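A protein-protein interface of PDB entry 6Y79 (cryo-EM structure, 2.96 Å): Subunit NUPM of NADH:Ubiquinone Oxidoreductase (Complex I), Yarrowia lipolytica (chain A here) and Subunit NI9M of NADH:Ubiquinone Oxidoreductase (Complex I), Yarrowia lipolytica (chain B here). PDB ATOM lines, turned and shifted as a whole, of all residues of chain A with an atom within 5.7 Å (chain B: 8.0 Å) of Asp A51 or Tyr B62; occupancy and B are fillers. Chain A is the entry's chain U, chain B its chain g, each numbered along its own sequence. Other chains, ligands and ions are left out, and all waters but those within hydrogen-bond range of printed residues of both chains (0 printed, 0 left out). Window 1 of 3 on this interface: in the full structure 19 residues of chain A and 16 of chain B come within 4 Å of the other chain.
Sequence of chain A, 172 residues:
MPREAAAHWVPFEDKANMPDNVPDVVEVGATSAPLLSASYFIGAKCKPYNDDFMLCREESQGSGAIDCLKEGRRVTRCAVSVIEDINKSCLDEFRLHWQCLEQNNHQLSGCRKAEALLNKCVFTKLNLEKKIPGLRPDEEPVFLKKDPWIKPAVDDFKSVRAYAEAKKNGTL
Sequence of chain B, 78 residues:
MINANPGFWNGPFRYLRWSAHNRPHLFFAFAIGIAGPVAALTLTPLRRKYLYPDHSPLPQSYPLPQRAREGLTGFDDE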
ATOM      1  N   CYS A  46       3.851  34.709   6.464  1.00  0.00           N
ATOM      2  CA  CYS A  46       4.160  33.286   6.528  1.00  0.00           C
ATOM      3  C   CYS A  46       4.759  32.856   7.860  1.00  0.00           C
ATOM      4  O   CYS A  46       5.588  31.946   7.883  1.00  0.00           O
ATOM      5  CB  CYS A  46       5.117  32.903   5.405  1.00  0.00           C
ATOM      6  SG  CYS A  46       4.461  33.098   3.759  1.00  0.00           S
ATOM      7  N   LYS A  47       4.369  33.482   8.966  1.00  0.00           N
ATOM      8  CA  LYS A  47       4.865  33.033  10.267  1.00  0.00           C
ATOM      9  C   LYS A  47       4.398  31.632  10.665  1.00  0.00           C
ATOM     10  O   LYS A  47       5.270  30.813  11.017  1.00  0.00           O
ATOM     11  CB  LYS A  47       4.547  34.078  11.345  1.00  0.00           C
ATOM     12  CG  LYS A  47       5.079  33.721  12.721  1.00  0.00           C
ATOM     13  CD  LYS A  47       4.731  34.794  13.732  1.00  0.00           C
ATOM     14  CE  LYS A  47       5.397  34.545  15.081  1.00  0.00           C
ATOM     15  NZ  LYS A  47       4.822  33.386  15.816  1.00  0.00           N
ATOM     16  N   PRO A  48       3.093  31.269  10.640  1.00  0.00           N
ATOM     17  CA  PRO A  48       2.744  29.902  11.071  1.00  0.00           C
ATOM     18  C   PRO A  48       3.195  28.814  10.111  1.00  0.00           C
ATOM     19  O   PRO A  48       3.475  27.702  10.567  1.00  0.00           O
ATOM     20  CB  PRO A  48       1.217  29.945  11.194  1.00  0.00           C
ATOM     21  CG  PRO A  48       0.809  30.951  10.241  1.00  0.00           C
ATOM     22  CD  PRO A  48       1.852  32.014  10.301  1.00  0.00           C
ATOM     23  N   TYR A  49       3.350  29.117   8.821  1.00  0.00           N
ATOM     24  CA  TYR A  49       3.842  28.122   7.873  1.00  0.00           C
ATOM     25  C   TYR A  49       5.322  27.831   8.097  1.00  0.00           C
ATOM     26  O   TYR A  49       5.733  26.664   8.151  1.00  0.00           O
ATOM     27  CB  TYR A  49       3.603  28.593   6.439  1.00  0.00           C
ATOM     28  CG  TYR A  49       2.146  28.789   6.107  1.00  0.00           C
ATOM     29  CD1 TYR A  49       1.530  30.011   6.327  1.00  0.00           C
ATOM     30  CD2 TYR A  49       1.385  27.752   5.581  1.00  0.00           C
ATOM     31  CE1 TYR A  49       0.207  30.200   6.040  1.00  0.00           C
ATOM     32  CE2 TYR A  49       0.050  27.935   5.286  1.00  0.00           C
ATOM     33  CZ  TYR A  49      -0.526  29.165   5.521  1.00  0.00           C
ATOM     34  OH  TYR A  49      -1.847  29.390   5.242  1.00  0.00           O
ATOM     35  N   ASN A  50       6.135  28.892   8.218  1.00  0.00           N
ATOM     36  CA  ASN A  50       7.560  28.741   8.507  1.00  0.00           C
ATOM     37  C   ASN A  50       7.784  28.045   9.839  1.00  0.00           C
ATOM     38  O   ASN A  50       8.680  27.198   9.971  1.00  0.00           O
ATOM     39  CB  ASN A  50       8.249  30.107   8.530  1.00  0.00           C
ATOM     40  CG  ASN A  50       8.356  30.738   7.164  1.00  0.00           C
ATOM     41  OD1 ASN A  50       8.601  30.064   6.168  1.00  0.00           O
ATOM     42  ND2 ASN A  50       8.184  32.052   7.113  1.00  0.00           N
ATOM     43  N   ASP A  51       6.959  28.370  10.832  1.00  0.00           N
ATOM     44  CA  ASP A  51       7.155  27.766  12.138  1.00  0.00           C
ATOM     45  C   ASP A  51       6.681  26.321  12.163  1.00  0.00           C
ATOM     46  O   ASP A  51       7.263  25.498  12.873  1.00  0.00           O
ATOM     47  CB  ASP A  51       6.476  28.602  13.207  1.00  0.00           C
ATOM     48  CG  ASP A  51       7.371  29.709  13.698  1.00  0.00           C
ATOM     49  OD1 ASP A  51       8.580  29.447  13.872  1.00  0.00           O
ATOM     50  OD2 ASP A  51       6.885  30.840  13.888  1.00  0.00           O
ATOM     51  N   ASP A  52       5.671  25.969  11.359  1.00  0.00           N
ATOM     52  CA  ASP A  52       5.308  24.563  11.242  1.00  0.00           C
ATOM     53  C   ASP A  52       6.392  23.783  10.514  1.00  0.00           C
ATOM     54  O   ASP A  52       6.641  22.622  10.840  1.00  0.00           O
ATOM     55  CB  ASP A  52       3.957  24.409  10.538  1.00  0.00           C
ATOM     56  CG  ASP A  52       3.257  23.088  10.868  1.00  0.00           C
ATOM     57  OD1 ASP A  52       3.888  22.017  10.822  1.00  0.00           O
ATOM     58  OD2 ASP A  52       2.044  23.111  11.157  1.00  0.00           O
ATOM     59  N   PHE A  53       7.081  24.411   9.556  1.00  0.00           N
ATOM     60  CA  PHE A  53       8.161  23.709   8.862  1.00  0.00           C
ATOM     61  C   PHE A  53       9.336  23.428   9.793  1.00  0.00           C
ATOM     62  O   PHE A  53       9.855  22.303   9.846  1.00  0.00           O
ATOM     63  CB  PHE A  53       8.639  24.508   7.656  1.00  0.00           C
ATOM     64  CG  PHE A  53       9.826  23.903   6.988  1.00  0.00           C
ATOM     65  CD1 PHE A  53       9.733  22.661   6.394  1.00  0.00           C
ATOM     66  CD2 PHE A  53      11.039  24.559   6.970  1.00  0.00           C
ATOM     67  CE1 PHE A  53      10.825  22.089   5.782  1.00  0.00           C
ATOM     68  CE2 PHE A  53      12.135  23.991   6.361  1.00  0.00           C
ATOM     69  CZ  PHE A  53      12.027  22.755   5.766  1.00  0.00           C
ATOM     70  N   MET A  54       9.764  24.436  10.552  1.00  0.00           N
ATOM     71  CA  MET A  54      10.867  24.193  11.475  1.00  0.00           C
ATOM     72  C   MET A  54      10.449  23.337  12.666  1.00  0.00           C
ATOM     73  O   MET A  54      11.280  22.600  13.207  1.00  0.00           O
ATOM     74  CB  MET A  54      11.474  25.519  11.932  1.00  0.00           C
ATOM     75  CG  MET A  54      12.085  26.329  10.800  1.00  0.00           C
ATOM     76  SD  MET A  54      13.153  25.384   9.695  1.00  0.00           S
ATOM     77  CE  MET A  54      14.716  25.442  10.548  1.00  0.00           C
ATOM     78  N   LEU A  55       9.167  23.356  13.032  1.00  0.00           N
ATOM     79  CA  LEU A  55       8.658  22.462  14.061  1.00  0.00           C
ATOM     80  C   LEU A  55       8.594  21.021  13.566  1.00  0.00           C
ATOM     81  O   LEU A  55       8.789  20.092  14.355  1.00  0.00           O
ATOM     82  CB  LEU A  55       7.290  22.967  14.504  1.00  0.00           C
ATOM     83  CG  LEU A  55       6.652  22.635  15.842  1.00  0.00           C
ATOM     84  CD1 LEU A  55       7.592  22.940  16.972  1.00  0.00           C
ATOM     85  CD2 LEU A  55       5.397  23.468  15.974  1.00  0.00           C
ATOM     86  N   CYS A  56       8.309  20.821  12.273  1.00  0.00           N
ATOM     87  CA  CYS A  56       8.454  19.512  11.649  1.00  0.00           C
ATOM     88  C   CYS A  56       9.879  19.028  11.760  1.00  0.00           C
ATOM     89  O   CYS A  56      10.130  17.869  12.103  1.00  0.00           O
ATOM     90  CB  CYS A  56       8.048  19.585  10.175  1.00  0.00           C
ATOM     91  SG  CYS A  56       8.373  18.083   9.179  1.00  0.00           S
ATOM     92  N   PRO B  59      18.391  37.362  19.042  1.00  0.00           N
ATOM     93  CA  PRO B  59      18.334  35.946  18.684  1.00  0.00           C
ATOM     94  C   PRO B  59      19.639  35.480  18.055  1.00  0.00           C
ATOM     95  O   PRO B  59      20.397  36.254  17.472  1.00  0.00           O
ATOM     96  CB  PRO B  59      17.167  35.876  17.695  1.00  0.00           C
ATOM     97  CG  PRO B  59      17.006  37.277  17.195  1.00  0.00           C
ATOM     98  CD  PRO B  59      17.341  38.135  18.364  1.00  0.00           C
ATOM     99  N   GLN B  60      19.905  34.190  18.216  1.00  0.00           N
ATOM    100  CA  GLN B  60      21.124  33.557  17.738  1.00  0.00           C
ATOM    101  C   GLN B  60      20.877  32.434  16.751  1.00  0.00           C
ATOM    102  O   GLN B  60      21.725  32.183  15.895  1.00  0.00           O
ATOM    103  CB  GLN B  60      21.925  33.001  18.913  1.00  0.00           C
ATOM    104  CG  GLN B  60      22.512  34.057  19.799  1.00  0.00           C
ATOM    105  CD  GLN B  60      22.998  33.475  21.098  1.00  0.00           C
ATOM    106  OE1 GLN B  60      22.733  32.314  21.404  1.00  0.00           O
ATOM    107  NE2 GLN B  60      23.719  34.270  21.869  1.00  0.00           N
ATOM    108  N   SER B  61      19.735  31.768  16.834  1.00  0.00           N
ATOM    109  CA  SER B  61      19.388  30.702  15.917  1.00  0.00           C
ATOM    110  C   SER B  61      18.052  31.044  15.283  1.00  0.00           C
ATOM    111  O   SER B  61      17.569  32.166  15.441  1.00  0.00           O
ATOM    112  CB  SER B  61      19.313  29.380  16.666  1.00  0.00           C
ATOM    113  OG  SER B  61      18.283  29.433  17.638  1.00  0.00           O
ATOM    114  N   TYR B  62      17.451  30.119  14.559  1.00  0.00           N
ATOM    115  CA  TYR B  62      16.030  30.258  14.309  1.00  0.00           C
ATOM    116  C   TYR B  62      15.296  30.013  15.621  1.00  0.00           C
ATOM    117  O   TYR B  62      15.589  29.032  16.313  1.00  0.00           O
ATOM    118  CB  TYR B  62      15.525  29.291  13.245  1.00  0.00           C
ATOM    119  CG  TYR B  62      14.071  29.524  12.907  1.00  0.00           C
ATOM    120  CD1 TYR B  62      13.697  30.526  12.025  1.00  0.00           C
ATOM    121  CD2 TYR B  62      13.071  28.755  13.487  1.00  0.00           C
ATOM    122  CE1 TYR B  62      12.370  30.748  11.724  1.00  0.00           C
ATOM    123  CE2 TYR B  62      11.748  28.978  13.203  1.00  0.00           C
ATOM    124  CZ  TYR B  62      11.403  29.969  12.317  1.00  0.00           C
ATOM    125  OH  TYR B  62      10.081  30.184  12.021  1.00  0.00           O
ATOM    126  N   PRO B  63      14.355  30.861  15.995  1.00  0.00           N
ATOM    127  CA  PRO B  63      13.589  30.619  17.219  1.00  0.00           C
ATOM    128  C   PRO B  63      12.550  29.523  17.049  1.00  0.00           C
ATOM    129  O   PRO B  63      11.521  29.715  16.393  1.00  0.00           O
ATOM    130  CB  PRO B  63      12.940  31.980  17.496  1.00  0.00           C
ATOM    131  CG  PRO B  63      12.868  32.644  16.180  1.00  0.00           C
ATOM    132  CD  PRO B  63      13.996  32.131  15.354  1.00  0.00           C
ATOM    133  N   LEU B  64      12.812  28.369  17.626  1.00  0.00           N
ATOM    134  CA  LEU B  64      11.809  27.313  17.633  1.00  0.00           C
ATOM    135  C   LEU B  64      10.853  27.525  18.793  1.00  0.00           C
ATOM    136  O   LEU B  64      11.301  27.643  19.937  1.00  0.00           O
ATOM    137  CB  LEU B  64      12.451  25.945  17.777  1.00  0.00           C
ATOM    138  CG  LEU B  64      13.289  25.363  16.651  1.00  0.00           C
ATOM    139  CD1 LEU B  64      13.959  24.099  17.144  1.00  0.00           C
ATOM    140  CD2 LEU B  64      12.408  25.068  15.469  1.00  0.00           C
ATOM    141  N   PRO B  65       9.548  27.583  18.556  1.00  0.00           N
ATOM    142  CA  PRO B  65       8.610  27.483  19.678  1.00  0.00           C
ATOM    143  C   PRO B  65       8.348  26.025  20.013  1.00  0.00           C
ATOM    144  O   PRO B  65       8.904  25.133  19.367  1.00  0.00           O
ATOM    145  CB  PRO B  65       7.361  28.198  19.156  1.00  0.00           C
ATOM    146  CG  PRO B  65       7.416  27.995  17.683  1.00  0.00           C
ATOM    147  CD  PRO B  65       8.869  27.919  17.292  1.00  0.00           C
ATOM    148  N   ARG B  67       5.489  23.567  20.188  1.00  0.00           N
ATOM    149  CA  ARG B  67       4.119  23.205  19.845  1.00  0.00           C
ATOM    150  C   ARG B  67       4.171  21.877  19.097  1.00  0.00           C
ATOM    151  O   ARG B  67       5.200  21.197  19.077  1.00  0.00           O
ATOM    152  CB  ARG B  67       3.436  24.310  19.025  1.00  0.00           C
ATOM    153  CG  ARG B  67       3.343  25.668  19.711  1.00  0.00           C
ATOM    154  CD  ARG B  67       2.373  26.587  19.002  1.00  0.00           C
ATOM    155  NE  ARG B  67       2.995  27.290  17.887  1.00  0.00           N
ATOM    156  CZ  ARG B  67       2.868  26.920  16.620  1.00  0.00           C
ATOM    157  NH1 ARG B  67       2.144  25.854  16.314  1.00  0.00           N
ATOM    158  NH2 ARG B  67       3.461  27.615  15.660  1.00  0.00           N
ATOM    159  N   ARG B  69       2.704  21.175  15.725  1.00  0.00           N
ATOM    160  CA  ARG B  69       2.362  21.284  14.298  1.00  0.00           C
ATOM    161  C   ARG B  69       0.857  21.235  14.057  1.00  0.00           C
ATOM    162  O   ARG B  69       0.352  20.347  13.367  1.00  0.00           O
ATOM    163  CB  ARG B  69       3.046  20.201  13.467  1.00  0.00           C
ATOM    164  CG  ARG B  69       4.539  20.209  13.481  1.00  0.00           C
ATOM    165  CD  ARG B  69       5.022  18.998  12.716  1.00  0.00           C
ATOM    166  NE  ARG B  69       4.479  18.901  11.366  1.00  0.00           N
ATOM    167  CZ  ARG B  69       4.798  17.934  10.512  1.00  0.00           C
ATOM    168  NH1 ARG B  69       4.262  17.900   9.301  1.00  0.00           N
ATOM    169  NH2 ARG B  69       5.646  16.984  10.877  1.00  0.00           N
ATOM    170  N   LEU B  72      -3.169  23.752   9.700  1.00  0.00           N
ATOM    171  CA  LEU B  72      -3.527  25.044   9.142  1.00  0.00           C
ATOM    172  C   LEU B  72      -4.069  24.838   7.742  1.00  0.00           C
ATOM    173  O   LEU B  72      -3.414  24.211   6.904  1.00  0.00           O
ATOM    174  CB  LEU B  72      -2.320  25.957   9.095  1.00  0.00           C
ATOM    175  CG  LEU B  72      -1.733  26.224  10.466  1.00  0.00           C
ATOM    176  CD1 LEU B  72      -0.390  26.809  10.182  1.00  0.00           C
ATOM    177  CD2 LEU B  72      -2.618  27.195  11.232  1.00  0.00           C
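The guanidinium group (NH2) of Arg B69 lies within hydrogen-bond range of the side-chain sulfur (SG) of Cys A56 (3.4 Å). The side-chain carboxylate (OD1) of Asp A52 is in salt-bridge range of the guanidinium group (NE) of Arg B69 (3.2 Å). The side-chain hydroxyl of Tyr B62 is in hydrogen-bond range of the side-chain carboxylate of Asp A51.
The side-chain carboxylate (OD2) of Asp A51 is in salt-bridge range of the side-chain amino group (NZ) of Lys A47 (3.8 Å). The backbone carbonyl oxygen (O) of Cys A46 is in hydrogen-bond range of the side-chain amide nitrogen (ND2) of Asn A50, 2.7 Å away.
Printed residues of chain B within 4 Å of Asn A50: Tyr B62 (3.8 Å). Of the printed residues of chain B, Asp A51 touches Tyr B62, Pro B63 and Pro B65. Tyr B62 touches just these residues of chain A: Asn A50, Asp A51 and Met A54. Of the printed residues of chain A, Pro B63 touches Asp A51. Printed residues of chain A within 4 Å of Pro B65: Asp A51 (3.8 Å) and Leu A55 (3.5 Å). Of the printed residues of chain A, Leu B72 touches Pro A48. The nearest printed residue of chain B that does not touch Pro A48 is Arg B67 (5.1 Å).
Leu B72 touches Pro A48. C of Asn A50 touches OH of Tyr B62 (3.8 Å). OD1 of Asp A51 touches O of Pro B63, 3.9 Å away. Pro B65 touches Asp A51. Tyr B62 touches Met A54. Met A54 touches Leu B64 (O to CD2, 3.5 Å). Pro B65 touches Leu A55. Arg B67 touches Leu A55 (O to CD1, 3.6 Å). CD2 of Leu A55 touches N of Arg B69, at 3.5 Å.
Hydrophobic or aromatic side chains of chain A that line the printed part of chain B: Pro A48, Met A54 and Leu A55.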
